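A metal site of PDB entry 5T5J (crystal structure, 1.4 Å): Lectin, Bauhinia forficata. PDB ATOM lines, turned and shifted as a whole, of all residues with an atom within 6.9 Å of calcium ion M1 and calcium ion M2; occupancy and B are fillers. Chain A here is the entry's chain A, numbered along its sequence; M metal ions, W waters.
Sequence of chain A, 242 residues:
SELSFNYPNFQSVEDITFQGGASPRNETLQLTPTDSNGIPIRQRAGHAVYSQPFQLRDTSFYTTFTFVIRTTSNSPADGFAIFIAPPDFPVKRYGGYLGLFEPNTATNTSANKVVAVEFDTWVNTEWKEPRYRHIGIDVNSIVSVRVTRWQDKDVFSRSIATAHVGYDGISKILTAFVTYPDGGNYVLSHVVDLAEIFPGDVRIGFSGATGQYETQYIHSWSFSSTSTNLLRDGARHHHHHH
Within 4 Å of calcium ion M1: Asp 120, Trp 122, Asn 124 and Glu 129.
Water W1 bridges the side-chain carboxylate (OE1) of Glu 118 (2.7 Å) and the backbone carbonyl oxygen (O) of Ile 142 (2.8 Å).
The nearest printed residue that does not touch calcium ion M2 is Ser 144 (4.3 Å).
Calcium ion M2 is bound by the side-chain carboxylate of Glu 129, the side-chain carboxylate of Asp 120, water W4, the side-chain carboxylate of Glu 118, water W1 and a ring nitrogen (NE2) of His 134.
The side-chain carboxylate (OE1) of Glu 118 lies close to the side-chain carboxylate (OD2) of Asp 138 (2.5 Å). The indole nitrogen of Trp 127 lies close to the side-chain carboxylate of Glu 129 (3.4 Å). N of Glu 118 lies within hydrogen-bond range of O of Gly 136.
Calcium ion M1 is bound by the backbone carbonyl oxygen (O) of Trp 122 (2.3 Å). The side-chain amide oxygen (OD1) of Asn 124 binds calcium ion M1, at 2.3 Å. OE2 of Glu 129 is bound to calcium ion M1. Calcium ion M1 is bound by water W2 (2.4 Å). Water W3 is bound to calcium ion M1 (2.4 Å). Calcium ion M1 is bound by OD2 of Asp 120, at 2.4 Å. Calcium ion M1 is bound by the side-chain carboxylate (OD1) of Asp 120, 2.5 Å away. Calcium ion M1 has seven donor atoms within binding distance.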
ATOM      1  N   ASP A  78      31.393  -4.479  11.592  1.00  0.00           N
ATOM      2  CA  ASP A  78      30.784  -3.598  10.547  1.00  0.00           C
ATOM      3  C   ASP A  78      29.888  -2.477  11.084  1.00  0.00           C
ATOM      4  O   ASP A  78      29.603  -1.560  10.316  1.00  0.00           O
ATOM      5  CB  ASP A  78      29.903  -4.508   9.664  1.00  0.00           C
ATOM      6  CG  ASP A  78      30.788  -5.133   8.593  1.00  0.00           C
ATOM      7  OD1 ASP A  78      31.014  -4.501   7.553  1.00  0.00           O
ATOM      8  OD2 ASP A  78      31.251  -6.291   8.841  1.00  0.00           O
ATOM      9  N   GLY A  95      28.473  -9.223   8.317  1.00  0.00           N
ATOM     10  CA  GLY A  95      29.262  -8.321   7.531  1.00  0.00           C
ATOM     11  C   GLY A  95      28.514  -7.036   7.250  1.00  0.00           C
ATOM     12  O   GLY A  95      27.736  -6.513   8.092  1.00  0.00           O
ATOM     13  N   GLY A  96      28.740  -6.479   6.055  1.00  0.00           N
ATOM     14  CA  GLY A  96      28.240  -5.162   5.728  1.00  0.00           C
ATOM     15  C   GLY A  96      26.757  -5.041   5.592  1.00  0.00           C
ATOM     16  O   GLY A  96      26.229  -3.916   5.582  1.00  0.00           O
ATOM     17  N   TYR A  97      26.080  -6.158   5.515  1.00  0.00           N
ATOM     18  CA  TYR A  97      24.613  -6.164   5.533  1.00  0.00           C
ATOM     19  C   TYR A  97      24.052  -5.865   6.884  1.00  0.00           C
ATOM     20  O   TYR A  97      22.812  -5.693   6.988  1.00  0.00           O
ATOM     21  CB  TYR A  97      24.127  -7.523   4.989  1.00  0.00           C
ATOM     22  CG  TYR A  97      24.697  -7.859   3.669  1.00  0.00           C
ATOM     23  CD1 TYR A  97      24.162  -7.285   2.519  1.00  0.00           C
ATOM     24  CD2 TYR A  97      25.760  -8.767   3.489  1.00  0.00           C
ATOM     25  CE1 TYR A  97      24.730  -7.531   1.277  1.00  0.00           C
ATOM     26  CE2 TYR A  97      26.288  -8.993   2.251  1.00  0.00           C
ATOM     27  CZ  TYR A  97      25.808  -8.416   1.132  1.00  0.00           C
ATOM     28  OH  TYR A  97      26.345  -8.686  -0.104  1.00  0.00           O
ATOM     29  N   LEU A  98      24.865  -5.852   7.917  1.00  0.00           N
ATOM     30  CA  LEU A  98      24.461  -5.351   9.232  1.00  0.00           C
ATOM     31  C   LEU A  98      23.401  -6.164   9.914  1.00  0.00           C
ATOM     32  O   LEU A  98      22.752  -5.674  10.821  1.00  0.00           O
ATOM     33  CB  LEU A  98      24.091  -3.841   9.256  1.00  0.00           C
ATOM     34  CG  LEU A  98      25.233  -2.894   8.912  1.00  0.00           C
ATOM     35  CD1 LEU A  98      24.747  -1.460   8.832  1.00  0.00           C
ATOM     36  CD2 LEU A  98      26.360  -2.966   9.903  1.00  0.00           C
ATOM     37  N   GLU A 118      21.663   3.519  10.968  1.00  0.00           N
ATOM     38  CA  GLU A 118      22.895   2.703  11.014  1.00  0.00           C
ATOM     39  C   GLU A 118      24.101   3.523  11.470  1.00  0.00           C
ATOM     40  O   GLU A 118      24.200   4.737  11.174  1.00  0.00           O
ATOM     41  CB  GLU A 118      23.207   2.045   9.661  1.00  0.00           C
ATOM     42  CG  GLU A 118      23.474   3.052   8.552  1.00  0.00           C
ATOM     43  CD  GLU A 118      24.120   2.379   7.324  1.00  0.00           C
ATOM     44  OE1 GLU A 118      23.513   1.343   6.849  1.00  0.00           O
ATOM     45  OE2 GLU A 118      25.193   2.792   6.876  1.00  0.00           O
ATOM     46  N   PHE A 119      24.996   2.828  12.121  1.00  0.00           N
ATOM     47  CA  PHE A 119      26.245   3.332  12.651  1.00  0.00           C
ATOM     48  C   PHE A 119      27.319   2.439  11.976  1.00  0.00           C
ATOM     49  O   PHE A 119      27.509   1.270  12.410  1.00  0.00           O
ATOM     50  CB  PHE A 119      26.287   3.198  14.173  1.00  0.00           C
ATOM     51  CG  PHE A 119      25.213   4.023  14.848  1.00  0.00           C
ATOM     52  CD1 PHE A 119      23.894   3.580  14.872  1.00  0.00           C
ATOM     53  CD2 PHE A 119      25.472   5.249  15.406  1.00  0.00           C
ATOM     54  CE1 PHE A 119      22.904   4.336  15.443  1.00  0.00           C
ATOM     55  CE2 PHE A 119      24.484   5.985  16.036  1.00  0.00           C
ATOM     56  CZ  PHE A 119      23.184   5.538  15.957  1.00  0.00           C
ATOM     57  N   ASP A 120      27.880   2.907  10.887  1.00  0.00           N
ATOM     58  CA  ASP A 120      28.630   2.060   9.942  1.00  0.00           C
ATOM     59  C   ASP A 120      30.126   2.286  10.079  1.00  0.00           C
ATOM     60  O   ASP A 120      30.583   3.360   9.747  1.00  0.00           O
ATOM     61  CB  ASP A 120      28.086   2.341   8.524  1.00  0.00           C
ATOM     62  CG  ASP A 120      28.590   1.336   7.475  1.00  0.00           C
ATOM     63  OD1 ASP A 120      29.632   0.719   7.771  1.00  0.00           O
ATOM     64  OD2 ASP A 120      27.921   1.183   6.423  1.00  0.00           O
ATOM     65  N   THR A 121      30.834   1.248  10.526  1.00  0.00           N
ATOM     66  CA  THR A 121      32.273   1.340  10.817  1.00  0.00           C
ATOM     67  C   THR A 121      33.158   0.894   9.671  1.00  0.00           C
ATOM     68  O   THR A 121      34.385   1.047   9.784  1.00  0.00           O
ATOM     69  CB  THR A 121      32.639   0.552  12.080  1.00  0.00           C
ATOM     70  OG1 THR A 121      32.351  -0.816  11.835  1.00  0.00           O
ATOM     71  CG2 THR A 121      31.915   1.020  13.336  1.00  0.00           C
ATOM     72  N   TRP A 122      32.617   0.366   8.577  1.00  0.00           N
ATOM     73  CA  TRP A 122      33.404  -0.244   7.520  1.00  0.00           C
ATOM     74  C   TRP A 122      32.838   0.214   6.164  1.00  0.00           C
ATOM     75  O   TRP A 122      31.665  -0.025   5.807  1.00  0.00           O
ATOM     76  CB  TRP A 122      33.375  -1.769   7.618  1.00  0.00           C
ATOM     77  CG  TRP A 122      34.075  -2.444   6.455  1.00  0.00           C
ATOM     78  CD1 TRP A 122      33.513  -2.666   5.237  1.00  0.00           C
ATOM     79  CD2 TRP A 122      35.405  -2.966   6.404  1.00  0.00           C
ATOM     80  NE1 TRP A 122      34.423  -3.297   4.377  1.00  0.00           N
ATOM     81  CE2 TRP A 122      35.581  -3.469   5.096  1.00  0.00           C
ATOM     82  CE3 TRP A 122      36.455  -3.000   7.299  1.00  0.00           C
ATOM     83  CZ2 TRP A 122      36.772  -4.084   4.653  1.00  0.00           C
ATOM     84  CZ3 TRP A 122      37.647  -3.668   6.852  1.00  0.00           C
ATOM     85  CH2 TRP A 122      37.762  -4.197   5.581  1.00  0.00           C
ATOM     86  N   VAL A 123      33.691   0.901   5.380  1.00  0.00           N
ATOM     87  CA  VAL A 123      33.287   1.364   4.077  1.00  0.00           C
ATOM     88  C   VAL A 123      33.262   0.154   3.111  1.00  0.00           C
ATOM     89  O   VAL A 123      34.301  -0.382   2.726  1.00  0.00           O
ATOM     90  CB  VAL A 123      34.230   2.465   3.600  1.00  0.00           C
ATOM     91  CG1 VAL A 123      33.940   2.913   2.115  1.00  0.00           C
ATOM     92  CG2 VAL A 123      34.216   3.672   4.492  1.00  0.00           C
ATOM     93  N   ASN A 124      32.085  -0.234   2.673  1.00  0.00           N
ATOM     94  CA  ASN A 124      31.928  -1.365   1.796  1.00  0.00           C
ATOM     95  C   ASN A 124      32.188  -0.953   0.353  1.00  0.00           C
ATOM     96  O   ASN A 124      31.701   0.081  -0.099  1.00  0.00           O
ATOM     97  CB  ASN A 124      30.534  -1.948   1.923  1.00  0.00           C
ATOM     98  CG  ASN A 124      30.469  -2.800   3.156  1.00  0.00           C
ATOM     99  OD1 ASN A 124      30.087  -2.326   4.240  1.00  0.00           O
ATOM    100  ND2 ASN A 124      30.832  -4.063   3.038  1.00  0.00           N
ATOM    101  N   TRP A 127      28.774  -1.932  -2.621  1.00  0.00           N
ATOM    102  CA  TRP A 127      27.653  -1.074  -2.959  1.00  0.00           C
ATOM    103  C   TRP A 127      28.101   0.371  -2.639  1.00  0.00           C
ATOM    104  O   TRP A 127      29.187   0.564  -2.020  1.00  0.00           O
ATOM    105  CB  TRP A 127      26.378  -1.444  -2.214  1.00  0.00           C
ATOM    106  CG  TRP A 127      26.552  -1.558  -0.727  1.00  0.00           C
ATOM    107  CD1 TRP A 127      26.558  -0.555   0.185  1.00  0.00           C
ATOM    108  CD2 TRP A 127      26.762  -2.741  -0.006  1.00  0.00           C
ATOM    109  NE1 TRP A 127      26.776  -1.051   1.453  1.00  0.00           N
ATOM    110  CE2 TRP A 127      26.929  -2.419   1.351  1.00  0.00           C
ATOM    111  CE3 TRP A 127      26.818  -4.080  -0.400  1.00  0.00           C
ATOM    112  CZ2 TRP A 127      27.143  -3.371   2.327  1.00  0.00           C
ATOM    113  CZ3 TRP A 127      27.053  -5.042   0.579  1.00  0.00           C
ATOM    114  CH2 TRP A 127      27.211  -4.658   1.939  1.00  0.00           C
ATOM    115  N   LYS A 128      27.281   1.362  -3.064  1.00  0.00           N
ATOM    116  CA  LYS A 128      27.644   2.738  -2.861  1.00  0.00           C
ATOM    117  C   LYS A 128      27.585   3.072  -1.375  1.00  0.00           C
ATOM    118  O   LYS A 128      26.548   2.958  -0.755  1.00  0.00           O
ATOM    119  CB  LYS A 128      26.625   3.638  -3.648  1.00  0.00           C
ATOM    120  CG  LYS A 128      26.781   5.139  -3.476  1.00  0.00           C
ATOM    121  CD  LYS A 128      25.648   5.901  -4.223  1.00  0.00           C
ATOM    122  CE  LYS A 128      24.638   6.509  -3.254  1.00  0.00           C
ATOM    123  NZ  LYS A 128      25.081   7.900  -2.919  1.00  0.00           N
ATOM    124  N   GLU A 129      28.727   3.519  -0.830  1.00  0.00           N
ATOM    125  CA  GLU A 129      28.920   4.076   0.479  1.00  0.00           C
ATOM    126  C   GLU A 129      29.809   5.261   0.414  1.00  0.00           C
ATOM    127  O   GLU A 129      30.688   5.258  -0.414  1.00  0.00           O
ATOM    128  CB  GLU A 129      29.720   3.013   1.456  1.00  0.00           C
ATOM    129  CG  GLU A 129      29.011   1.755   1.619  1.00  0.00           C
ATOM    130  CD  GLU A 129      28.745   1.350   3.060  1.00  0.00           C
ATOM    131  OE1 GLU A 129      27.587   1.537   3.422  1.00  0.00           O
ATOM    132  OE2 GLU A 129      29.672   0.904   3.741  1.00  0.00           O
ATOM    133  N   PRO A 130      29.648   6.239   1.352  1.00  0.00           N
ATOM    134  CA  PRO A 130      30.676   7.288   1.382  1.00  0.00           C
ATOM    135  C   PRO A 130      32.000   6.701   1.789  1.00  0.00           C
ATOM    136  O   PRO A 130      32.030   5.694   2.485  1.00  0.00           O
ATOM    137  CB  PRO A 130      30.159   8.246   2.444  1.00  0.00           C
ATOM    138  CG  PRO A 130      29.092   7.583   3.154  1.00  0.00           C
ATOM    139  CD  PRO A 130      28.605   6.397   2.392  1.00  0.00           C
ATOM    140  N   HIS A 134      30.323   6.371   8.816  1.00  0.00           N
ATOM    141  CA  HIS A 134      29.157   7.212   8.629  1.00  0.00           C
ATOM    142  C   HIS A 134      27.973   6.743   9.498  1.00  0.00           C
ATOM    143  O   HIS A 134      27.895   5.542   9.822  1.00  0.00           O
ATOM    144  CB  HIS A 134      28.780   7.289   7.138  1.00  0.00           C
ATOM    145  CG  HIS A 134      28.609   5.970   6.473  1.00  0.00           C
ATOM    146  ND1 HIS A 134      29.694   5.259   5.963  1.00  0.00           N
ATOM    147  CD2 HIS A 134      27.536   5.211   6.200  1.00  0.00           C
ATOM    148  CE1 HIS A 134      29.289   4.110   5.484  1.00  0.00           C
ATOM    149  NE2 HIS A 134      27.979   4.074   5.586  1.00  0.00           N
ATOM    150  N   GLY A 136      23.763   6.748   9.024  1.00  0.00           N
ATOM    151  CA  GLY A 136      22.843   6.840   7.926  1.00  0.00           C
ATOM    152  C   GLY A 136      21.428   6.451   8.298  1.00  0.00           C
ATOM    153  O   GLY A 136      21.201   5.691   9.229  1.00  0.00           O
ATOM    154  N   ASP A 138      18.490   4.263   6.537  1.00  0.00           N
ATOM    155  CA  ASP A 138      18.251   3.240   5.543  1.00  0.00           C
ATOM    156  C   ASP A 138      16.767   2.977   5.386  1.00  0.00           C
ATOM    157  O   ASP A 138      16.077   2.751   6.390  1.00  0.00           O
ATOM    158  CB  ASP A 138      18.912   1.944   5.982  1.00  0.00           C
ATOM    159  CG  ASP A 138      20.381   2.039   6.116  1.00  0.00           C
ATOM    160  OD1 ASP A 138      20.996   3.010   5.672  1.00  0.00           O
ATOM    161  OD2 ASP A 138      20.982   1.122   6.807  1.00  0.00           O
ATOM    162  N   ILE A 142      20.434  -1.313   1.865  1.00  0.00           N
ATOM    163  CA  ILE A 142      21.697  -1.081   2.560  1.00  0.00           C
ATOM    164  C   ILE A 142      22.413   0.175   2.116  1.00  0.00           C
ATOM    165  O   ILE A 142      23.347   0.653   2.763  1.00  0.00           O
ATOM    166  CB  ILE A 142      22.570  -2.362   2.477  1.00  0.00           C
ATOM    167  CG1 ILE A 142      23.686  -2.376   3.513  1.00  0.00           C
ATOM    168  CG2 ILE A 142      23.137  -2.549   1.082  1.00  0.00           C
ATOM    169  CD1 ILE A 142      23.320  -2.254   5.015  1.00  0.00           C
ATOM    170  N   VAL A 143      22.012   0.742   0.970  1.00  0.00           N
ATOM    171  CA  VAL A 143      22.513   2.054   0.505  1.00  0.00           C
ATOM    172  C   VAL A 143      21.687   3.132   1.151  1.00  0.00           C
ATOM    173  O   VAL A 143      20.498   3.246   0.803  1.00  0.00           O
ATOM    174  CB  VAL A 143      22.503   2.136  -1.053  1.00  0.00           C
ATOM    175  CG1 VAL A 143      22.871   3.602  -1.524  1.00  0.00           C
ATOM    176  CG2 VAL A 143      23.429   1.076  -1.650  1.00  0.00           C
ATOM    177  N   SER A 144      22.256   3.861   2.082  1.00  0.00           N
ATOM    178  CA  SER A 144      21.498   4.832   2.843  1.00  0.00           C
ATOM    179  C   SER A 144      20.883   5.949   1.968  1.00  0.00           C
ATOM    180  O   SER A 144      21.532   6.374   1.019  1.00  0.00           O
ATOM    181  CB  SER A 144      22.403   5.484   3.866  1.00  0.00           C
ATOM    182  OG  SER A 144      22.968   4.585   4.759  1.00  0.00           O
ATOM    183  N   VAL A 147      23.000  10.276   4.653  1.00  0.00           N
ATOM    184  CA  VAL A 147      24.180   9.791   5.299  1.00  0.00           C
ATOM    185  C   VAL A 147      25.004  10.985   5.741  1.00  0.00           C
ATOM    186  O   VAL A 147      25.033  12.013   5.040  1.00  0.00           O
ATOM    187  CB  VAL A 147      24.840   8.774   4.393  1.00  0.00           C
ATOM    188  CG1 VAL A 147      25.491   9.440   3.184  1.00  0.00           C
ATOM    189  CG2 VAL A 147      25.678   7.849   5.027  1.00  0.00           C
HETATM  190 CA    CA M   1      29.436  -0.557   5.632  1.00  0.00          CA
HETATM  191 CA    CA M   2      26.547   2.281   5.164  1.00  0.00          CA
HETATM  192  O   HOH W   1      25.137   0.500   4.896  1.00  0.00           O
HETATM  193  O   HOH W   2      29.683  -2.141   7.422  1.00  0.00           O
HETATM  194  O   HOH W   3      27.229  -1.414   5.221  1.00  0.00           O
HETATM  195  O   HOH W   4      25.358   3.602   3.905  1.00  0.00           O
